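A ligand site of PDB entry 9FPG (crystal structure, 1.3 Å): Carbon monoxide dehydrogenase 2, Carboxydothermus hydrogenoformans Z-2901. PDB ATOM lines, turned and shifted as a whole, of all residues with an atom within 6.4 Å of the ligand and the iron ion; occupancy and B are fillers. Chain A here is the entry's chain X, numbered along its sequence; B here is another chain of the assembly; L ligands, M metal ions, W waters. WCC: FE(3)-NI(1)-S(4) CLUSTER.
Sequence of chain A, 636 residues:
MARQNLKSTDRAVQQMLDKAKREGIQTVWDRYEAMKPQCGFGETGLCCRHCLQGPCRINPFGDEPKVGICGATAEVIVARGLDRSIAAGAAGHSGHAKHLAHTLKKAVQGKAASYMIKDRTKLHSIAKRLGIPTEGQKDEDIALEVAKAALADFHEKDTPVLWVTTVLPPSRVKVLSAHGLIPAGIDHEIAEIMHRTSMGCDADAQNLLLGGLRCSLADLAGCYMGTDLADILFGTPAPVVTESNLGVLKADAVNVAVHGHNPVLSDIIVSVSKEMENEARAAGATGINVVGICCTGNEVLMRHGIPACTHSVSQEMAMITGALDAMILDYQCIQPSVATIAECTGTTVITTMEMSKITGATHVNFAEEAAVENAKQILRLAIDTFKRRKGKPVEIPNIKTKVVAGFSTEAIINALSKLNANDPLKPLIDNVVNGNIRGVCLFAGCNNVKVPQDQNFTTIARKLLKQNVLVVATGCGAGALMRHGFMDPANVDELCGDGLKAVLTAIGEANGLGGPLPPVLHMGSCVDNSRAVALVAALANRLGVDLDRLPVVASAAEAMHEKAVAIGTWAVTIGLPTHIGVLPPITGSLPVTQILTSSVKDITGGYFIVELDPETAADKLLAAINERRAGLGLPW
O of Gly 445 lies close to S1 of the ligand (3.4 Å).
CB of Cys 294 touches S3 of the ligand, 3.7 Å away.
CE of Met 560 touches S2 of the ligand, at 3.7 Å.
His 561 touches the ligand.
Hydrophobic or aromatic side chains that line the ligand: His 261, Met 560 and His 561.
Of the 29 residues printed, 12 come within 4 Å of the ligand.
The nearest printed residue that does not touch the ligand is Gly 475 (4.4 Å).
The iron ion is bound by water W2 (2.0 Å), a ring nitrogen (NE2) of His 261 (2.1 Å), the side-chain sulfur of Cys 295 (2.3 Å) and a sulfur (S3) of the ligand (2.4 Å).
The iron ion has four donor atoms within binding distance.
Water W1 bridges O of Cys 333 (2.8 Å) and S2 of the ligand (3.5 Å).
The backbone carbonyl oxygen (O) of Met 199 of chain B sits at hydrogen-bond distance from the backbone NH (N) of Cys 333, 3.2 Å away.
SG of Cys 446 sits close to N of Met 560 (3.4 Å).
The backbone NH of Cys 476 sits close to the backbone carbonyl oxygen of Gly 445 (3.3 Å).
The side-chain sulfur (SG) of Cys 294 is in hydrogen-bond range of the backbone NH (N) of Ser 312.
The backbone NH of Asn 447 is in hydrogen-bond range of the side-chain hydroxyl of Ser 312 (3.1 Å).
The backbone NH (N) of Lys 563 lies within hydrogen-bond range of a ring nitrogen (ND1) of His 561 (2.9 Å).
NZ of Lys 563 lies within hydrogen-bond range of OE1 of Gln 332 (2.8 Å).
NE2 of His 561 sits at hydrogen-bond distance from O of Met 199 of chain B (2.9 Å).
Residues that only touch the iron ion: Cys 526 (3.3 Å) and Lys 563 (3.6 Å).
A nickel atom (NI) of the ligand is bound by the side-chain sulfur of Cys 526 (2.0 Å).
An iron atom (FE1) of the ligand is bound by the side-chain sulfur (SG) of Cys 333, at 2.2 Å.
A sulfur (S1) of the ligand lies close to the backbone NH (N) of Cys 446 (3.7 Å).
SG of Cys 446 is bound to FE3 of the ligand, at 2.3 Å.
A sulfur (S1) of the ligand lies close to the backbone NH (N) of Cys 476 (3.6 Å).
The side-chain sulfur (SG) of Cys 476 binds an iron atom (FE4) of the ligand.
The side-chain hydroxyl (OG) of Ser 312 lies close to a sulfur (S2) of the ligand.
S4 of the ligand lies close to NZ of Lys 563.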
ATOM      1  N   HIS A  93     -10.182  24.765  10.641  1.00  0.00           N
ATOM      2  CA  HIS A  93      -9.981  25.173   9.262  1.00  0.00           C
ATOM      3  C   HIS A  93      -8.712  26.003   9.100  1.00  0.00           C
ATOM      4  O   HIS A  93      -8.120  25.983   8.011  1.00  0.00           O
ATOM      5  CB  HIS A  93     -11.224  25.913   8.771  1.00  0.00           C
ATOM      6  CG  HIS A  93     -12.381  24.997   8.549  1.00  0.00           C
ATOM      7  ND1 HIS A  93     -13.666  25.308   8.952  1.00  0.00           N
ATOM      8  CD2 HIS A  93     -12.456  23.772   7.961  1.00  0.00           C
ATOM      9  CE1 HIS A  93     -14.474  24.318   8.613  1.00  0.00           C
ATOM     10  NE2 HIS A  93     -13.771  23.372   8.011  1.00  0.00           N
ATOM     11  N   GLY A 260     -10.260  11.531   7.904  1.00  0.00           N
ATOM     12  CA  GLY A 260      -9.737  12.810   8.346  1.00  0.00           C
ATOM     13  C   GLY A 260     -10.039  13.860   7.305  1.00  0.00           C
ATOM     14  O   GLY A 260     -11.155  13.859   6.760  1.00  0.00           O
ATOM     15  N   HIS A 261      -9.061  14.715   6.975  1.00  0.00           N
ATOM     16  CA  HIS A 261      -9.365  15.956   6.252  1.00  0.00           C
ATOM     17  C   HIS A 261      -8.477  16.380   5.104  1.00  0.00           C
ATOM     18  O   HIS A 261      -9.005  16.866   4.088  1.00  0.00           O
ATOM     19  CB  HIS A 261      -9.576  17.106   7.250  1.00  0.00           C
ATOM     20  CG  HIS A 261     -10.920  17.021   7.877  1.00  0.00           C
ATOM     21  ND1 HIS A 261     -11.192  16.095   8.860  1.00  0.00           N
ATOM     22  CD2 HIS A 261     -12.110  17.541   7.501  1.00  0.00           C
ATOM     23  CE1 HIS A 261     -12.492  16.111   9.124  1.00  0.00           C
ATOM     24  NE2 HIS A 261     -13.062  16.979   8.302  1.00  0.00           N
ATOM     25  N   CYS A 294     -15.321  10.238   5.604  1.00  0.00           N
ATOM     26  CA  CYS A 294     -15.343  11.644   6.051  1.00  0.00           C
ATOM     27  C   CYS A 294     -14.779  12.533   4.936  1.00  0.00           C
ATOM     28  O   CYS A 294     -14.847  12.172   3.741  1.00  0.00           O
ATOM     29  CB  CYS A 294     -14.717  11.816   7.432  1.00  0.00           C
ATOM     30  SG  CYS A 294     -15.805  11.357   8.784  1.00  0.00           S
ATOM     31  N   CYS A 295     -14.228  13.689   5.314  1.00  0.00           N
ATOM     32  CA  CYS A 295     -13.940  14.730   4.321  1.00  0.00           C
ATOM     33  C   CYS A 295     -12.796  14.339   3.407  1.00  0.00           C
ATOM     34  O   CYS A 295     -12.853  14.625   2.207  1.00  0.00           O
ATOM     35  CB  CYS A 295     -13.596  16.060   5.005  1.00  0.00           C
ATOM     36  SG  CYS A 295     -14.982  17.135   5.390  1.00  0.00           S
ATOM     37  N   THR A 296     -11.718  13.763   3.950  1.00  0.00           N
ATOM     38  CA  THR A 296     -10.617  13.415   3.073  1.00  0.00           C
ATOM     39  C   THR A 296     -11.044  12.349   2.066  1.00  0.00           C
ATOM     40  O   THR A 296     -10.563  12.342   0.923  1.00  0.00           O
ATOM     41  CB  THR A 296      -9.360  13.061   3.869  1.00  0.00           C
ATOM     42  OG1 THR A 296      -8.197  13.317   3.054  1.00  0.00           O
ATOM     43  CG2 THR A 296      -9.362  11.626   4.295  1.00  0.00           C
ATOM     44  N   HIS A 311     -19.294   7.461   6.518  1.00  0.00           N
ATOM     45  CA  HIS A 311     -19.114   8.818   6.990  1.00  0.00           C
ATOM     46  C   HIS A 311     -19.486   8.959   8.457  1.00  0.00           C
ATOM     47  O   HIS A 311     -20.351   8.245   8.960  1.00  0.00           O
ATOM     48  CB  HIS A 311     -20.017   9.786   6.241  1.00  0.00           C
ATOM     49  CG  HIS A 311     -19.857   9.715   4.770  1.00  0.00           C
ATOM     50  ND1 HIS A 311     -20.525   8.806   3.989  1.00  0.00           N
ATOM     51  CD2 HIS A 311     -19.044  10.416   3.931  1.00  0.00           C
ATOM     52  CE1 HIS A 311     -20.157   8.951   2.731  1.00  0.00           C
ATOM     53  NE2 HIS A 311     -19.256   9.928   2.672  1.00  0.00           N
ATOM     54  N   SER A 312     -18.828   9.920   9.105  1.00  0.00           N
ATOM     55  CA  SER A 312     -19.248  10.499  10.367  1.00  0.00           C
ATOM     56  C   SER A 312     -19.578   9.448  11.408  1.00  0.00           C
ATOM     57  O   SER A 312     -18.723   8.621  11.776  1.00  0.00           O
ATOM     58  CB  SER A 312     -20.425  11.452  10.052  1.00  0.00           C
ATOM     59  OG  SER A 312     -20.760  12.321  11.118  1.00  0.00           O
ATOM     60  N   VAL A 313     -20.824   9.457  11.882  1.00  0.00           N
ATOM     61  CA  VAL A 313     -21.200   8.687  13.068  1.00  0.00           C
ATOM     62  C   VAL A 313     -20.982   7.195  12.887  1.00  0.00           C
ATOM     63  O   VAL A 313     -20.717   6.486  13.871  1.00  0.00           O
ATOM     64  CB  VAL A 313     -22.642   9.040  13.454  1.00  0.00           C
ATOM     65  CG1 VAL A 313     -23.636   8.471  12.433  1.00  0.00           C
ATOM     66  CG2 VAL A 313     -22.949   8.545  14.852  1.00  0.00           C
ATOM     67  N   GLN A 332      -9.243  15.553  12.675  1.00  0.00           N
ATOM     68  CA  GLN A 332     -10.612  16.056  12.780  1.00  0.00           C
ATOM     69  C   GLN A 332     -11.659  14.991  12.463  1.00  0.00           C
ATOM     70  O   GLN A 332     -11.598  14.338  11.408  1.00  0.00           O
ATOM     71  CB  GLN A 332     -10.877  17.274  11.885  1.00  0.00           C
ATOM     72  CG  GLN A 332      -9.975  18.469  12.136  1.00  0.00           C
ATOM     73  CD  GLN A 332     -10.044  19.495  11.024  1.00  0.00           C
ATOM     74  OE1 GLN A 332     -10.964  19.509  10.207  1.00  0.00           O
ATOM     75  NE2 GLN A 332      -9.039  20.366  10.977  1.00  0.00           N
ATOM     76  N   CYS A 333     -12.621  14.821  13.370  1.00  0.00           N
ATOM     77  CA  CYS A 333     -13.817  14.004  13.166  1.00  0.00           C
ATOM     78  C   CYS A 333     -13.546  12.510  13.247  1.00  0.00           C
ATOM     79  O   CYS A 333     -14.431  11.715  12.893  1.00  0.00           O
ATOM     80  CB  CYS A 333     -14.550  14.381  11.874  1.00  0.00           C
ATOM     81  SG  CYS A 333     -14.992  16.124  11.918  1.00  0.00           S
ATOM     82  N   ALA A 444     -25.244  20.595   4.565  1.00  0.00           N
ATOM     83  CA  ALA A 444     -23.873  20.652   5.025  1.00  0.00           C
ATOM     84  C   ALA A 444     -23.762  19.974   6.375  1.00  0.00           C
ATOM     85  O   ALA A 444     -24.761  19.721   7.052  1.00  0.00           O
ATOM     86  CB  ALA A 444     -23.373  22.095   5.113  1.00  0.00           C
ATOM     87  N   GLY A 445     -22.524  19.673   6.771  1.00  0.00           N
ATOM     88  CA  GLY A 445     -22.272  19.223   8.112  1.00  0.00           C
ATOM     89  C   GLY A 445     -22.409  17.724   8.305  1.00  0.00           C
ATOM     90  O   GLY A 445     -22.457  16.918   7.363  1.00  0.00           O
ATOM     91  N   CYS A 446     -22.546  17.366   9.575  1.00  0.00           N
ATOM     92  CA  CYS A 446     -22.265  16.039  10.097  1.00  0.00           C
ATOM     93  C   CYS A 446     -23.518  15.191  10.216  1.00  0.00           C
ATOM     94  O   CYS A 446     -24.631  15.644   9.916  1.00  0.00           O
ATOM     95  CB  CYS A 446     -21.661  16.214  11.508  1.00  0.00           C
ATOM     96  SG  CYS A 446     -20.643  17.741  11.784  1.00  0.00           S
ATOM     97  N   ASN A 447     -23.341  13.922  10.627  1.00  0.00           N
ATOM     98  CA  ASN A 447     -24.337  13.151  11.372  1.00  0.00           C
ATOM     99  C   ASN A 447     -24.095  13.393  12.865  1.00  0.00           C
ATOM    100  O   ASN A 447     -23.012  13.833  13.285  1.00  0.00           O
ATOM    101  CB  ASN A 447     -24.236  11.629  11.129  1.00  0.00           C
ATOM    102  CG  ASN A 447     -24.453  11.201   9.684  1.00  0.00           C
ATOM    103  OD1 ASN A 447     -23.595  10.524   9.104  1.00  0.00           O
ATOM    104  ND2 ASN A 447     -25.616  11.519   9.119  1.00  0.00           N
ATOM    105  N   THR A 474     -22.465  19.035   0.690  1.00  0.00           N
ATOM    106  CA  THR A 474     -21.045  18.883   0.980  1.00  0.00           C
ATOM    107  C   THR A 474     -20.879  18.009   2.223  1.00  0.00           C
ATOM    108  O   THR A 474     -21.810  17.737   2.972  1.00  0.00           O
ATOM    109  CB  THR A 474     -20.406  20.235   1.288  1.00  0.00           C
ATOM    110  OG1 THR A 474     -21.017  20.749   2.467  1.00  0.00           O
ATOM    111  CG2 THR A 474     -20.550  21.193   0.130  1.00  0.00           C
ATOM    112  N   GLY A 475     -19.637  17.590   2.439  1.00  0.00           N
ATOM    113  CA  GLY A 475     -19.272  16.937   3.679  1.00  0.00           C
ATOM    114  C   GLY A 475     -20.082  15.685   3.917  1.00  0.00           C
ATOM    115  O   GLY A 475     -20.355  14.897   3.000  1.00  0.00           O
ATOM    116  N   CYS A 476     -20.458  15.459   5.171  1.00  0.00           N
ATOM    117  CA  CYS A 476     -21.244  14.287   5.540  1.00  0.00           C
ATOM    118  C   CYS A 476     -22.726  14.463   5.271  1.00  0.00           C
ATOM    119  O   CYS A 476     -23.494  13.509   5.369  1.00  0.00           O
ATOM    120  CB  CYS A 476     -20.870  13.875   6.971  1.00  0.00           C
ATOM    121  SG  CYS A 476     -19.070  13.426   7.121  1.00  0.00           S
ATOM    122  N   GLY A 477     -23.149  15.663   4.846  1.00  0.00           N
ATOM    123  CA  GLY A 477     -24.464  15.816   4.261  1.00  0.00           C
ATOM    124  C   GLY A 477     -24.484  15.206   2.865  1.00  0.00           C
ATOM    125  O   GLY A 477     -25.409  14.477   2.505  1.00  0.00           O
ATOM    126  N   SER A 525     -16.027  18.570  -0.077  1.00  0.00           N
ATOM    127  CA  SER A 525     -15.780  18.401   1.341  1.00  0.00           C
ATOM    128  C   SER A 525     -16.336  19.583   2.123  1.00  0.00           C
ATOM    129  O   SER A 525     -16.950  20.512   1.608  1.00  0.00           O
ATOM    130  CB  SER A 525     -14.290  18.379   1.589  1.00  0.00           C
ATOM    131  OG  SER A 525     -13.759  19.617   1.153  1.00  0.00           O
ATOM    132  N   CYS A 526     -16.099  19.598   3.441  1.00  0.00           N
ATOM    133  CA  CYS A 526     -16.640  20.694   4.256  1.00  0.00           C
ATOM    134  C   CYS A 526     -15.968  22.036   3.944  1.00  0.00           C
ATOM    135  O   CYS A 526     -16.634  23.078   3.945  1.00  0.00           O
ATOM    136  CB  CYS A 526     -16.545  20.370   5.757  1.00  0.00           C
ATOM    137  SG  CYS A 526     -17.601  19.021   6.396  1.00  0.00           S
ATOM    138  N   VAL A 527     -14.648  22.066   3.687  1.00  0.00           N
ATOM    139  CA  VAL A 527     -14.048  23.325   3.255  1.00  0.00           C
ATOM    140  C   VAL A 527     -14.703  23.785   1.962  1.00  0.00           C
ATOM    141  O   VAL A 527     -14.868  24.990   1.725  1.00  0.00           O
ATOM    142  CB  VAL A 527     -12.519  23.315   3.150  1.00  0.00           C
ATOM    143  CG1 VAL A 527     -11.883  23.218   4.535  1.00  0.00           C
ATOM    144  CG2 VAL A 527     -12.001  22.217   2.230  1.00  0.00           C
ATOM    145  N   ASN A 529     -17.717  23.843   1.231  1.00  0.00           N
ATOM    146  CA  ASN A 529     -18.823  24.775   1.377  1.00  0.00           C
ATOM    147  C   ASN A 529     -18.462  26.120   0.766  1.00  0.00           C
ATOM    148  O   ASN A 529     -19.345  26.860   0.319  1.00  0.00           O
ATOM    149  CB  ASN A 529     -19.197  24.925   2.850  1.00  0.00           C
ATOM    150  CG  ASN A 529     -19.983  23.758   3.352  1.00  0.00           C
ATOM    151  OD1 ASN A 529     -21.038  23.399   2.780  1.00  0.00           O
ATOM    152  ND2 ASN A 529     -19.468  23.097   4.385  1.00  0.00           N
ATOM    153  N   MET A 560     -22.843  18.373  14.300  1.00  0.00           N
ATOM    154  CA  MET A 560     -22.118  17.834  15.445  1.00  0.00           C
ATOM    155  C   MET A 560     -20.887  18.662  15.822  1.00  0.00           C
ATOM    156  O   MET A 560     -20.725  19.105  16.963  1.00  0.00           O
ATOM    157  CB  MET A 560     -21.708  16.388  15.139  1.00  0.00           C
ATOM    158  CG  MET A 560     -20.868  15.677  16.193  1.00  0.00           C
ATOM    159  SD  MET A 560     -19.078  15.814  16.028  1.00  0.00           S
ATOM    160  CE  MET A 560     -18.827  14.998  14.481  1.00  0.00           C
ATOM    161  N   HIS A 561     -19.992  18.883  14.869  1.00  0.00           N
ATOM    162  CA  HIS A 561     -18.673  19.408  15.190  1.00  0.00           C
ATOM    163  C   HIS A 561     -18.715  20.919  15.388  1.00  0.00           C
ATOM    164  O   HIS A 561     -19.584  21.618  14.875  1.00  0.00           O
ATOM    165  CB  HIS A 561     -17.712  19.072  14.049  1.00  0.00           C
ATOM    166  CG  HIS A 561     -16.277  19.083  14.444  1.00  0.00           C
ATOM    167  ND1 HIS A 561     -15.529  20.251  14.516  1.00  0.00           N
ATOM    168  CD2 HIS A 561     -15.436  18.086  14.801  1.00  0.00           C
ATOM    169  CE1 HIS A 561     -14.299  19.953  14.906  1.00  0.00           C
ATOM    170  NE2 HIS A 561     -14.217  18.644  15.077  1.00  0.00           N
ATOM    171  N   LYS A 563     -16.780  22.795  13.928  1.00  0.00           N
ATOM    172  CA  LYS A 563     -16.669  23.306  12.567  1.00  0.00           C
ATOM    173  C   LYS A 563     -18.031  23.525  11.934  1.00  0.00           C
ATOM    174  O   LYS A 563     -18.210  24.455  11.139  1.00  0.00           O
ATOM    175  CB  LYS A 563     -15.877  22.331  11.696  1.00  0.00           C
ATOM    176  CG  LYS A 563     -14.381  22.322  11.944  1.00  0.00           C
ATOM    177  CD  LYS A 563     -13.663  21.279  11.108  1.00  0.00           C
ATOM    178  CE  LYS A 563     -13.940  19.900  11.619  1.00  0.00           C
ATOM    179  NZ  LYS A 563     -13.701  18.917  10.500  1.00  0.00           N
ATOM    180  N   ALA A 564     -19.013  22.694  12.262  1.00  0.00           N
ATOM    181  CA  ALA A 564     -20.347  22.876  11.680  1.00  0.00           C
ATOM    182  C   ALA A 564     -21.058  24.083  12.273  1.00  0.00           C
ATOM    183  O   ALA A 564     -21.819  24.768  11.571  1.00  0.00           O
ATOM    184  CB  ALA A 564     -21.166  21.593  11.868  1.00  0.00           C
ATOM    185  N   ILE A 567     -19.527  27.002  10.404  1.00  0.00           N
ATOM    186  CA  ILE A 567     -20.083  27.095   9.049  1.00  0.00           C
ATOM    187  C   ILE A 567     -21.491  27.652   9.091  1.00  0.00           C
ATOM    188  O   ILE A 567     -21.861  28.524   8.299  1.00  0.00           O
ATOM    189  CB  ILE A 567     -20.035  25.737   8.343  1.00  0.00           C
ATOM    190  CG1 ILE A 567     -18.611  25.404   7.937  1.00  0.00           C
ATOM    191  CG2 ILE A 567     -20.993  25.749   7.114  1.00  0.00           C
ATOM    192  CD1 ILE A 567     -18.362  23.939   7.678  1.00  0.00           C
ATOM    193  N   MET B 199     -13.205  18.107  18.406  1.00  0.00           N
ATOM    194  CA  MET B 199     -13.642  16.720  18.359  1.00  0.00           C
ATOM    195  C   MET B 199     -12.887  15.951  17.282  1.00  0.00           C
ATOM    196  O   MET B 199     -12.691  16.437  16.151  1.00  0.00           O
ATOM    197  CB  MET B 199     -15.154  16.660  18.106  1.00  0.00           C
ATOM    198  CG  MET B 199     -15.769  15.265  18.082  1.00  0.00           C
ATOM    199  SD  MET B 199     -15.693  14.542  16.425  1.00  0.00           S
ATOM    200  CE  MET B 199     -16.615  13.020  16.653  1.00  0.00           C
HETATM  201 NI   WCC L   1     -17.498  18.589   8.389  1.00  0.00          NI
HETATM  202 FE1  WCC L   1     -16.571  16.107  10.355  1.00  0.00          FE
HETATM  203 FE3  WCC L   1     -18.961  17.074  10.312  1.00  0.00          FE
HETATM  204 FE4  WCC L   1     -18.219  15.137   8.526  1.00  0.00          FE
HETATM  205  S1  WCC L   1     -19.183  17.103   8.073  1.00  0.00           S
HETATM  206  S2  WCC L   1     -18.450  14.821  10.830  1.00  0.00           S
HETATM  207  S3  WCC L   1     -15.960  15.178   8.382  1.00  0.00           S
HETATM  208  S4  WCC L   1     -17.174  18.293  10.516  1.00  0.00           S
HETATM  209 FE    FE M   1     -15.078  17.243   7.664  1.00  0.00          FE
HETATM  210  O   HOH W   1     -17.160  12.184  12.663  1.00  0.00           O
HETATM  211  O   HOH W   2     -15.326  19.145   8.379  1.00  0.00           O
